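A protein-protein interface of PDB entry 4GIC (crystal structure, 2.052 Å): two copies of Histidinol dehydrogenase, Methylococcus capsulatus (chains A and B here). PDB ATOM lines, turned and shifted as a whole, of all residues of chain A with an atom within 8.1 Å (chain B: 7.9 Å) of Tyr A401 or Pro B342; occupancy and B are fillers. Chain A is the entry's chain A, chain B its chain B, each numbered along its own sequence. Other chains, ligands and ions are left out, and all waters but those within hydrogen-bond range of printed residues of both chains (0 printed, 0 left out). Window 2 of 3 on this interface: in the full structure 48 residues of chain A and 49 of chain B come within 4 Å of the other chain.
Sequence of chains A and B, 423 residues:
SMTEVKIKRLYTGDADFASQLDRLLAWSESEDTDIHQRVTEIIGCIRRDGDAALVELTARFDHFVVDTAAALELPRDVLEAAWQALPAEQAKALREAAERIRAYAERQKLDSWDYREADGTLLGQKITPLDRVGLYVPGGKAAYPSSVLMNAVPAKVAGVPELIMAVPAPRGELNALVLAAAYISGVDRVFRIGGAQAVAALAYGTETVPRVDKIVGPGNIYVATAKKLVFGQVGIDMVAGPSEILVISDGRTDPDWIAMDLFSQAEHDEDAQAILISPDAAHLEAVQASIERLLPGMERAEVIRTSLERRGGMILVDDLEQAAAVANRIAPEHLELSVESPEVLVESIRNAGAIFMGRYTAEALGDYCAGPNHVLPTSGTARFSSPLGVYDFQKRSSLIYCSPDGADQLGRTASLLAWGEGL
N of Met B357 sits at hydrogen-bond distance from O of Ile A400, 2.9 Å away. N of Ile B355 lies within hydrogen-bond range of O of Ser A398. The backbone NH of Ile A400 lies within hydrogen-bond range of the backbone carbonyl oxygen of Ile B355 (2.8 Å).
O of Leu A122 lies within hydrogen-bond range of N of Tyr A401, 2.8 Å away. O of Phe B356 sits at hydrogen-bond distance from N of Leu B337. N of Leu A399 sits at hydrogen-bond distance from O of Gly A124 (2.9 Å).
Leu A399 touches Ile B355 (CA to O, 3.4 Å). Ile A400 touches Phe B356 (O to CA, 3.5 Å). CG of Pro B342 touches OH of Tyr A401, 3.9 Å away. CD1 of Tyr A401 touches O of Met B357, at 3.2 Å.
Pro B342 touches just one residue of chain A: Tyr A401. Printed residues of chain B within 4 Å of Leu A399: Ile B355. Of the printed residues of chain A, Met B357 touches Ile A400 and Tyr A401. Ser B348 touches none of the printed residues of chain A. The nearest residue of chain B that does not touch Tyr A401 is Gly B358 (4.1 Å). The nearest printed residue of chain A that does not touch Pro B342 is Leu A399 (7.8 Å).
Hydrophobic or aromatic side chains of chain A within 4 Å of the printed part of chain B: Leu A399, Ile A400 and Tyr A401. Hydrophobic or aromatic side chains of chain B within 4 Å of the printed part of chain A: Pro B342, Ile B355, Phe B356 and Met B357. Among the printed residues, no Asp or Glu carboxylate lies within 4 Å of a Lys or Arg side-chain nitrogen of the other chain.
No position is printed for both chains. Of the 7 pairs that touch across the chains among the printed residues, none has its exchanged pair printed and touching as well.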
ATOM      1  N   TYR A 115     -16.463  32.244  27.815  1.00  0.00           N
ATOM      2  CA  TYR A 115     -16.922  32.582  29.152  1.00  0.00           C
ATOM      3  C   TYR A 115     -16.491  31.509  30.138  1.00  0.00           C
ATOM      4  O   TYR A 115     -16.091  30.404  29.732  1.00  0.00           O
ATOM      5  CB  TYR A 115     -18.434  32.756  29.199  1.00  0.00           C
ATOM      6  CG  TYR A 115     -19.220  31.492  28.932  1.00  0.00           C
ATOM      7  CD1 TYR A 115     -19.443  31.061  27.635  1.00  0.00           C
ATOM      8  CD2 TYR A 115     -19.746  30.735  29.973  1.00  0.00           C
ATOM      9  CE1 TYR A 115     -20.177  29.918  27.374  1.00  0.00           C
ATOM     10  CE2 TYR A 115     -20.483  29.585  29.721  1.00  0.00           C
ATOM     11  CZ  TYR A 115     -20.694  29.186  28.414  1.00  0.00           C
ATOM     12  OH  TYR A 115     -21.420  28.050  28.127  1.00  0.00           O
ATOM     13  N   GLY A 120     -15.261  27.260  37.009  1.00  0.00           N
ATOM     14  CA  GLY A 120     -14.050  27.833  36.446  1.00  0.00           C
ATOM     15  C   GLY A 120     -13.663  27.307  35.073  1.00  0.00           C
ATOM     16  O   GLY A 120     -12.739  27.824  34.439  1.00  0.00           O
ATOM     17  N   THR A 121     -14.401  26.311  34.593  1.00  0.00           N
ATOM     18  CA  THR A 121     -14.164  25.745  33.276  1.00  0.00           C
ATOM     19  C   THR A 121     -14.379  26.816  32.215  1.00  0.00           C
ATOM     20  O   THR A 121     -15.322  27.602  32.292  1.00  0.00           O
ATOM     21  CB  THR A 121     -15.101  24.551  33.002  1.00  0.00           C
ATOM     22  OG1 THR A 121     -14.908  23.552  34.010  1.00  0.00           O
ATOM     23  CG2 THR A 121     -14.829  23.950  31.612  1.00  0.00           C
ATOM     24  N   LEU A 122     -13.492  26.859  31.234  1.00  0.00           N
ATOM     25  CA  LEU A 122     -13.615  27.835  30.161  1.00  0.00           C
ATOM     26  C   LEU A 122     -14.304  27.216  28.962  1.00  0.00           C
ATOM     27  O   LEU A 122     -13.823  26.226  28.412  1.00  0.00           O
ATOM     28  CB  LEU A 122     -12.242  28.311  29.713  1.00  0.00           C
ATOM     29  CG  LEU A 122     -12.262  29.397  28.636  1.00  0.00           C
ATOM     30  CD1 LEU A 122     -12.064  30.789  29.241  1.00  0.00           C
ATOM     31  CD2 LEU A 122     -11.301  29.097  27.484  1.00  0.00           C
ATOM     32  N   LEU A 123     -15.412  27.807  28.531  1.00  0.00           N
ATOM     33  CA  LEU A 123     -16.065  27.344  27.320  1.00  0.00           C
ATOM     34  C   LEU A 123     -16.039  28.459  26.300  1.00  0.00           C
ATOM     35  O   LEU A 123     -16.144  29.629  26.657  1.00  0.00           O
ATOM     36  CB  LEU A 123     -17.501  26.936  27.607  1.00  0.00           C
ATOM     37  CG  LEU A 123     -17.645  25.787  28.596  1.00  0.00           C
ATOM     38  CD1 LEU A 123     -19.111  25.580  28.882  1.00  0.00           C
ATOM     39  CD2 LEU A 123     -17.013  24.529  28.023  1.00  0.00           C
ATOM     40  N   GLY A 124     -15.916  28.108  25.028  1.00  0.00           N
ATOM     41  CA  GLY A 124     -15.815  29.133  24.022  1.00  0.00           C
ATOM     42  C   GLY A 124     -16.195  28.710  22.625  1.00  0.00           C
ATOM     43  O   GLY A 124     -16.396  27.537  22.311  1.00  0.00           O
ATOM     44  N   SER A 398     -15.876  24.442  18.776  1.00  0.00           N
ATOM     45  CA  SER A 398     -16.043  24.524  20.233  1.00  0.00           C
ATOM     46  C   SER A 398     -14.699  24.469  20.975  1.00  0.00           C
ATOM     47  O   SER A 398     -13.835  23.641  20.647  1.00  0.00           O
ATOM     48  CB  SER A 398     -16.949  23.399  20.719  1.00  0.00           C
ATOM     49  OG  SER A 398     -18.203  23.483  20.068  1.00  0.00           O
ATOM     50  N   LEU A 399     -14.515  25.360  21.951  1.00  0.00           N
ATOM     51  CA  LEU A 399     -13.330  25.314  22.813  1.00  0.00           C
ATOM     52  C   LEU A 399     -13.730  24.934  24.245  1.00  0.00           C
ATOM     53  O   LEU A 399     -14.679  25.484  24.810  1.00  0.00           O
ATOM     54  CB  LEU A 399     -12.631  26.661  22.868  1.00  0.00           C
ATOM     55  CG  LEU A 399     -12.116  27.292  21.590  1.00  0.00           C
ATOM     56  CD1 LEU A 399     -11.497  28.627  21.930  1.00  0.00           C
ATOM     57  CD2 LEU A 399     -11.107  26.385  20.926  1.00  0.00           C
ATOM     58  N   ILE A 400     -12.983  24.004  24.826  1.00  0.00           N
ATOM     59  CA  ILE A 400     -13.173  23.588  26.211  1.00  0.00           C
ATOM     60  C   ILE A 400     -11.834  23.625  26.928  1.00  0.00           C
ATOM     61  O   ILE A 400     -10.882  22.959  26.498  1.00  0.00           O
ATOM     62  CB  ILE A 400     -13.725  22.153  26.314  1.00  0.00           C
ATOM     63  CG1 ILE A 400     -15.043  22.019  25.549  1.00  0.00           C
ATOM     64  CG2 ILE A 400     -13.942  21.782  27.766  1.00  0.00           C
ATOM     65  CD1 ILE A 400     -14.880  21.540  24.117  1.00  0.00           C
ATOM     66  N   TYR A 401     -11.733  24.461  27.960  1.00  0.00           N
ATOM     67  CA  TYR A 401     -10.533  24.518  28.796  1.00  0.00           C
ATOM     68  C   TYR A 401     -10.879  24.154  30.248  1.00  0.00           C
ATOM     69  O   TYR A 401     -10.507  23.084  30.743  1.00  0.00           O
ATOM     70  CB  TYR A 401      -9.895  25.906  28.730  1.00  0.00           C
ATOM     71  CG  TYR A 401      -8.423  25.934  29.079  1.00  0.00           C
ATOM     72  CD1 TYR A 401      -7.802  24.825  29.634  1.00  0.00           C
ATOM     73  CD2 TYR A 401      -7.648  27.064  28.831  1.00  0.00           C
ATOM     74  CE1 TYR A 401      -6.457  24.835  29.948  1.00  0.00           C
ATOM     75  CE2 TYR A 401      -6.295  27.086  29.141  1.00  0.00           C
ATOM     76  CZ  TYR A 401      -5.705  25.962  29.700  1.00  0.00           C
ATOM     77  OH  TYR A 401      -4.360  25.956  30.017  1.00  0.00           O
ATOM     78  N   ARG B 100     -25.402  22.802  31.282  1.00  0.00           N
ATOM     79  CA  ARG B 100     -24.218  23.295  30.556  1.00  0.00           C
ATOM     80  C   ARG B 100     -24.554  23.518  29.082  1.00  0.00           C
ATOM     81  O   ARG B 100     -24.271  24.592  28.496  1.00  0.00           O
ATOM     82  CB  ARG B 100     -23.059  22.295  30.675  1.00  0.00           C
ATOM     83  CG  ARG B 100     -22.304  22.350  32.003  1.00  0.00           C
ATOM     84  CD  ARG B 100     -21.434  21.098  32.213  1.00  0.00           C
ATOM     85  NE  ARG B 100     -20.255  21.011  31.349  1.00  0.00           N
ATOM     86  CZ  ARG B 100     -19.002  21.127  31.782  1.00  0.00           C
ATOM     87  NH1 ARG B 100     -18.753  21.313  33.071  1.00  0.00           N
ATOM     88  NH2 ARG B 100     -17.993  21.029  30.930  1.00  0.00           N
ATOM     89  N   ASP B 250       3.042  17.088  23.384  1.00  0.00           N
ATOM     90  CA  ASP B 250       4.411  17.596  23.439  1.00  0.00           C
ATOM     91  C   ASP B 250       5.369  16.603  24.107  1.00  0.00           C
ATOM     92  O   ASP B 250       6.586  16.781  24.066  1.00  0.00           O
ATOM     93  CB  ASP B 250       4.458  18.968  24.121  1.00  0.00           C
ATOM     94  CG  ASP B 250       4.006  18.922  25.572  1.00  0.00           C
ATOM     95  OD1 ASP B 250       3.570  17.853  26.047  1.00  0.00           O
ATOM     96  OD2 ASP B 250       4.063  19.972  26.239  1.00  0.00           O
ATOM     97  N   LEU B 320       5.849  21.292  16.977  1.00  0.00           N
ATOM     98  CA  LEU B 320       4.430  21.560  17.181  1.00  0.00           C
ATOM     99  C   LEU B 320       3.802  22.355  16.044  1.00  0.00           C
ATOM    100  O   LEU B 320       2.588  22.262  15.818  1.00  0.00           O
ATOM    101  CB  LEU B 320       4.183  22.244  18.527  1.00  0.00           C
ATOM    102  CG  LEU B 320       4.396  21.334  19.741  1.00  0.00           C
ATOM    103  CD1 LEU B 320       4.106  22.072  21.031  1.00  0.00           C
ATOM    104  CD2 LEU B 320       3.545  20.078  19.634  1.00  0.00           C
ATOM    105  N   GLU B 336      -7.464  17.362  20.712  1.00  0.00           N
ATOM    106  CA  GLU B 336      -6.912  17.577  22.044  1.00  0.00           C
ATOM    107  C   GLU B 336      -5.485  18.118  22.014  1.00  0.00           C
ATOM    108  O   GLU B 336      -4.574  17.480  21.479  1.00  0.00           O
ATOM    109  CB  GLU B 336      -6.907  16.282  22.855  1.00  0.00           C
ATOM    110  CG  GLU B 336      -6.321  16.477  24.238  1.00  0.00           C
ATOM    111  CD  GLU B 336      -6.819  15.463  25.231  1.00  0.00           C
ATOM    112  OE1 GLU B 336      -7.822  14.783  24.927  1.00  0.00           O
ATOM    113  OE2 GLU B 336      -6.194  15.337  26.305  1.00  0.00           O
ATOM    114  N   LEU B 337      -5.290  19.268  22.648  1.00  0.00           N
ATOM    115  CA  LEU B 337      -3.981  19.893  22.708  1.00  0.00           C
ATOM    116  C   LEU B 337      -3.322  19.570  24.039  1.00  0.00           C
ATOM    117  O   LEU B 337      -3.284  20.402  24.944  1.00  0.00           O
ATOM    118  CB  LEU B 337      -4.117  21.403  22.529  1.00  0.00           C
ATOM    119  CG  LEU B 337      -4.818  21.847  21.241  1.00  0.00           C
ATOM    120  CD1 LEU B 337      -4.967  23.362  21.216  1.00  0.00           C
ATOM    121  CD2 LEU B 337      -4.070  21.334  19.996  1.00  0.00           C
ATOM    122  N   SER B 338      -2.777  18.365  24.144  1.00  0.00           N
ATOM    123  CA  SER B 338      -2.123  17.938  25.377  1.00  0.00           C
ATOM    124  C   SER B 338      -0.687  18.448  25.363  1.00  0.00           C
ATOM    125  O   SER B 338       0.261  17.683  25.180  1.00  0.00           O
ATOM    126  CB  SER B 338      -2.169  16.413  25.515  1.00  0.00           C
ATOM    127  OG  SER B 338      -1.972  16.007  26.860  1.00  0.00           O
ATOM    128  N   VAL B 339      -0.552  19.764  25.539  1.00  0.00           N
ATOM    129  CA  VAL B 339       0.739  20.453  25.530  1.00  0.00           C
ATOM    130  C   VAL B 339       0.764  21.541  26.605  1.00  0.00           C
ATOM    131  O   VAL B 339      -0.280  21.888  27.171  1.00  0.00           O
ATOM    132  CB  VAL B 339       1.002  21.115  24.168  1.00  0.00           C
ATOM    133  CG1 VAL B 339       1.020  20.075  23.063  1.00  0.00           C
ATOM    134  CG2 VAL B 339      -0.060  22.185  23.889  1.00  0.00           C
ATOM    135  N   GLU B 340       1.945  22.106  26.851  1.00  0.00           N
ATOM    136  CA  GLU B 340       2.126  23.040  27.960  1.00  0.00           C
ATOM    137  C   GLU B 340       1.448  24.387  27.729  1.00  0.00           C
ATOM    138  O   GLU B 340       0.865  24.944  28.653  1.00  0.00           O
ATOM    139  CB  GLU B 340       3.608  23.248  28.262  1.00  0.00           C
ATOM    140  CG  GLU B 340       3.882  24.068  29.527  1.00  0.00           C
ATOM    141  CD  GLU B 340       3.526  23.328  30.821  1.00  0.00           C
ATOM    142  OE1 GLU B 340       3.396  22.084  30.795  1.00  0.00           O
ATOM    143  OE2 GLU B 340       3.390  23.992  31.871  1.00  0.00           O
ATOM    144  N   SER B 341       1.525  24.919  26.513  1.00  0.00           N
ATOM    145  CA  SER B 341       0.912  26.221  26.233  1.00  0.00           C
ATOM    146  C   SER B 341      -0.132  26.156  25.119  1.00  0.00           C
ATOM    147  O   SER B 341       0.070  26.701  24.029  1.00  0.00           O
ATOM    148  CB  SER B 341       1.983  27.266  25.906  1.00  0.00           C
ATOM    149  OG  SER B 341       2.745  27.588  27.061  1.00  0.00           O
ATOM    150  N   PRO B 342      -1.273  25.514  25.408  1.00  0.00           N
ATOM    151  CA  PRO B 342      -2.301  25.278  24.393  1.00  0.00           C
ATOM    152  C   PRO B 342      -2.990  26.567  23.973  1.00  0.00           C
ATOM    153  O   PRO B 342      -3.536  26.619  22.867  1.00  0.00           O
ATOM    154  CB  PRO B 342      -3.283  24.347  25.110  1.00  0.00           C
ATOM    155  CG  PRO B 342      -3.134  24.695  26.560  1.00  0.00           C
ATOM    156  CD  PRO B 342      -1.677  25.004  26.732  1.00  0.00           C
ATOM    157  N   GLU B 343      -2.987  27.581  24.836  1.00  0.00           N
ATOM    158  CA  GLU B 343      -3.614  28.857  24.490  1.00  0.00           C
ATOM    159  C   GLU B 343      -2.788  29.566  23.409  1.00  0.00           C
ATOM    160  O   GLU B 343      -3.290  30.438  22.698  1.00  0.00           O
ATOM    161  CB  GLU B 343      -3.773  29.752  25.724  1.00  0.00           C
ATOM    162  CG  GLU B 343      -2.513  30.525  26.098  1.00  0.00           C
ATOM    163  CD  GLU B 343      -1.481  29.682  26.833  1.00  0.00           C
ATOM    164  OE1 GLU B 343      -1.716  28.470  27.035  1.00  0.00           O
ATOM    165  OE2 GLU B 343      -0.424  30.234  27.204  1.00  0.00           O
ATOM    166  N   VAL B 344      -1.526  29.161  23.273  1.00  0.00           N
ATOM    167  CA  VAL B 344      -0.678  29.669  22.205  1.00  0.00           C
ATOM    168  C   VAL B 344      -0.830  28.790  20.960  1.00  0.00           C
ATOM    169  O   VAL B 344      -1.005  29.292  19.847  1.00  0.00           O
ATOM    170  CB  VAL B 344       0.800  29.724  22.639  1.00  0.00           C
ATOM    171  CG1 VAL B 344       1.683  30.132  21.476  1.00  0.00           C
ATOM    172  CG2 VAL B 344       0.972  30.688  23.803  1.00  0.00           C
ATOM    173  N   LEU B 345      -0.800  27.478  21.155  1.00  0.00           N
ATOM    174  CA  LEU B 345      -0.883  26.555  20.029  1.00  0.00           C
ATOM    175  C   LEU B 345      -2.193  26.697  19.264  1.00  0.00           C
ATOM    176  O   LEU B 345      -2.210  26.619  18.029  1.00  0.00           O
ATOM    177  CB  LEU B 345      -0.716  25.111  20.508  1.00  0.00           C
ATOM    178  CG  LEU B 345      -0.758  24.049  19.405  1.00  0.00           C
ATOM    179  CD1 LEU B 345       0.262  24.374  18.324  1.00  0.00           C
ATOM    180  CD2 LEU B 345      -0.510  22.638  19.972  1.00  0.00           C
ATOM    181  N   VAL B 346      -3.280  26.953  19.987  1.00  0.00           N
ATOM    182  CA  VAL B 346      -4.596  26.995  19.357  1.00  0.00           C
ATOM    183  C   VAL B 346      -4.676  28.100  18.293  1.00  0.00           C
ATOM    184  O   VAL B 346      -5.531  28.052  17.404  1.00  0.00           O
ATOM    185  CB  VAL B 346      -5.732  27.129  20.391  1.00  0.00           C
ATOM    186  CG1 VAL B 346      -5.810  28.551  20.918  1.00  0.00           C
ATOM    187  CG2 VAL B 346      -7.064  26.718  19.778  1.00  0.00           C
ATOM    188  N   GLU B 347      -3.773  29.078  18.376  1.00  0.00           N
ATOM    189  CA  GLU B 347      -3.719  30.157  17.393  1.00  0.00           C
ATOM    190  C   GLU B 347      -3.389  29.635  16.008  1.00  0.00           C
ATOM    191  O   GLU B 347      -3.730  30.266  15.009  1.00  0.00           O
ATOM    192  CB  GLU B 347      -2.667  31.193  17.781  1.00  0.00           C
ATOM    193  CG  GLU B 347      -2.887  31.844  19.125  1.00  0.00           C
ATOM    194  CD  GLU B 347      -4.163  32.654  19.161  1.00  0.00           C
ATOM    195  OE1 GLU B 347      -4.524  33.245  18.120  1.00  0.00           O
ATOM    196  OE2 GLU B 347      -4.802  32.712  20.233  1.00  0.00           O
ATOM    197  N   SER B 348      -2.744  28.474  15.952  1.00  0.00           N
ATOM    198  CA  SER B 348      -2.339  27.886  14.684  1.00  0.00           C
ATOM    199  C   SER B 348      -3.386  26.898  14.160  1.00  0.00           C
ATOM    200  O   SER B 348      -3.297  26.426  13.020  1.00  0.00           O
ATOM    201  CB  SER B 348      -1.004  27.172  14.858  1.00  0.00           C
ATOM    202  OG  SER B 348      -0.075  28.000  15.540  1.00  0.00           O
ATOM    203  N   ILE B 349      -4.391  26.611  14.985  1.00  0.00           N
ATOM    204  CA  ILE B 349      -5.424  25.642  14.625  1.00  0.00           C
ATOM    205  C   ILE B 349      -6.565  26.313  13.869  1.00  0.00           C
ATOM    206  O   ILE B 349      -7.139  27.284  14.360  1.00  0.00           O
ATOM    207  CB  ILE B 349      -5.998  24.934  15.893  1.00  0.00           C
ATOM    208  CG1 ILE B 349      -4.892  24.151  16.612  1.00  0.00           C
ATOM    209  CG2 ILE B 349      -7.213  24.046  15.543  1.00  0.00           C
ATOM    210  CD1 ILE B 349      -4.237  23.061  15.761  1.00  0.00           C
ATOM    211  N   ILE B 355     -12.228  21.699  20.353  1.00  0.00           N
ATOM    212  CA  ILE B 355     -10.843  21.714  20.814  1.00  0.00           C
ATOM    213  C   ILE B 355     -10.789  21.687  22.343  1.00  0.00           C
ATOM    214  O   ILE B 355     -11.371  22.545  23.028  1.00  0.00           O
ATOM    215  CB  ILE B 355     -10.079  22.936  20.296  1.00  0.00           C
ATOM    216  CG1 ILE B 355     -10.116  22.972  18.763  1.00  0.00           C
ATOM    217  CG2 ILE B 355      -8.636  22.913  20.789  1.00  0.00           C
ATOM    218  CD1 ILE B 355      -9.714  24.312  18.193  1.00  0.00           C
ATOM    219  N   PHE B 356     -10.115  20.666  22.860  1.00  0.00           N
ATOM    220  CA  PHE B 356      -9.940  20.461  24.284  1.00  0.00           C
ATOM    221  C   PHE B 356      -8.532  20.875  24.636  1.00  0.00           C
ATOM    222  O   PHE B 356      -7.564  20.312  24.108  1.00  0.00           O
ATOM    223  CB  PHE B 356     -10.134  18.989  24.626  1.00  0.00           C
ATOM    224  CG  PHE B 356     -11.463  18.457  24.210  1.00  0.00           C
ATOM    225  CD1 PHE B 356     -12.574  18.612  25.024  1.00  0.00           C
ATOM    226  CD2 PHE B 356     -11.612  17.834  22.981  1.00  0.00           C
ATOM    227  CE1 PHE B 356     -13.808  18.136  24.630  1.00  0.00           C
ATOM    228  CE2 PHE B 356     -12.842  17.358  22.577  1.00  0.00           C
ATOM    229  CZ  PHE B 356     -13.943  17.507  23.403  1.00  0.00           C
ATOM    230  N   MET B 357      -8.410  21.842  25.536  1.00  0.00           N
ATOM    231  CA  MET B 357      -7.098  22.321  25.927  1.00  0.00           C
ATOM    232  C   MET B 357      -6.802  21.941  27.362  1.00  0.00           C
ATOM    233  O   MET B 357      -7.693  21.967  28.209  1.00  0.00           O
ATOM    234  CB  MET B 357      -6.993  23.828  25.715  1.00  0.00           C
ATOM    235  CG  MET B 357      -7.160  24.212  24.261  1.00  0.00           C
ATOM    236  SD  MET B 357      -7.353  26.111  23.976  1.00  0.00           S
ATOM    237  CE  MET B 357      -8.970  26.421  25.002  1.00  0.00           C
ATOM    238  N   GLY B 358      -5.549  21.578  27.621  1.00  0.00           N
ATOM    239  CA  GLY B 358      -5.138  21.119  28.935  1.00  0.00           C
ATOM    240  C   GLY B 358      -5.136  19.603  28.970  1.00  0.00           C
ATOM    241  O   GLY B 358      -5.233  18.962  27.920  1.00  0.00           O
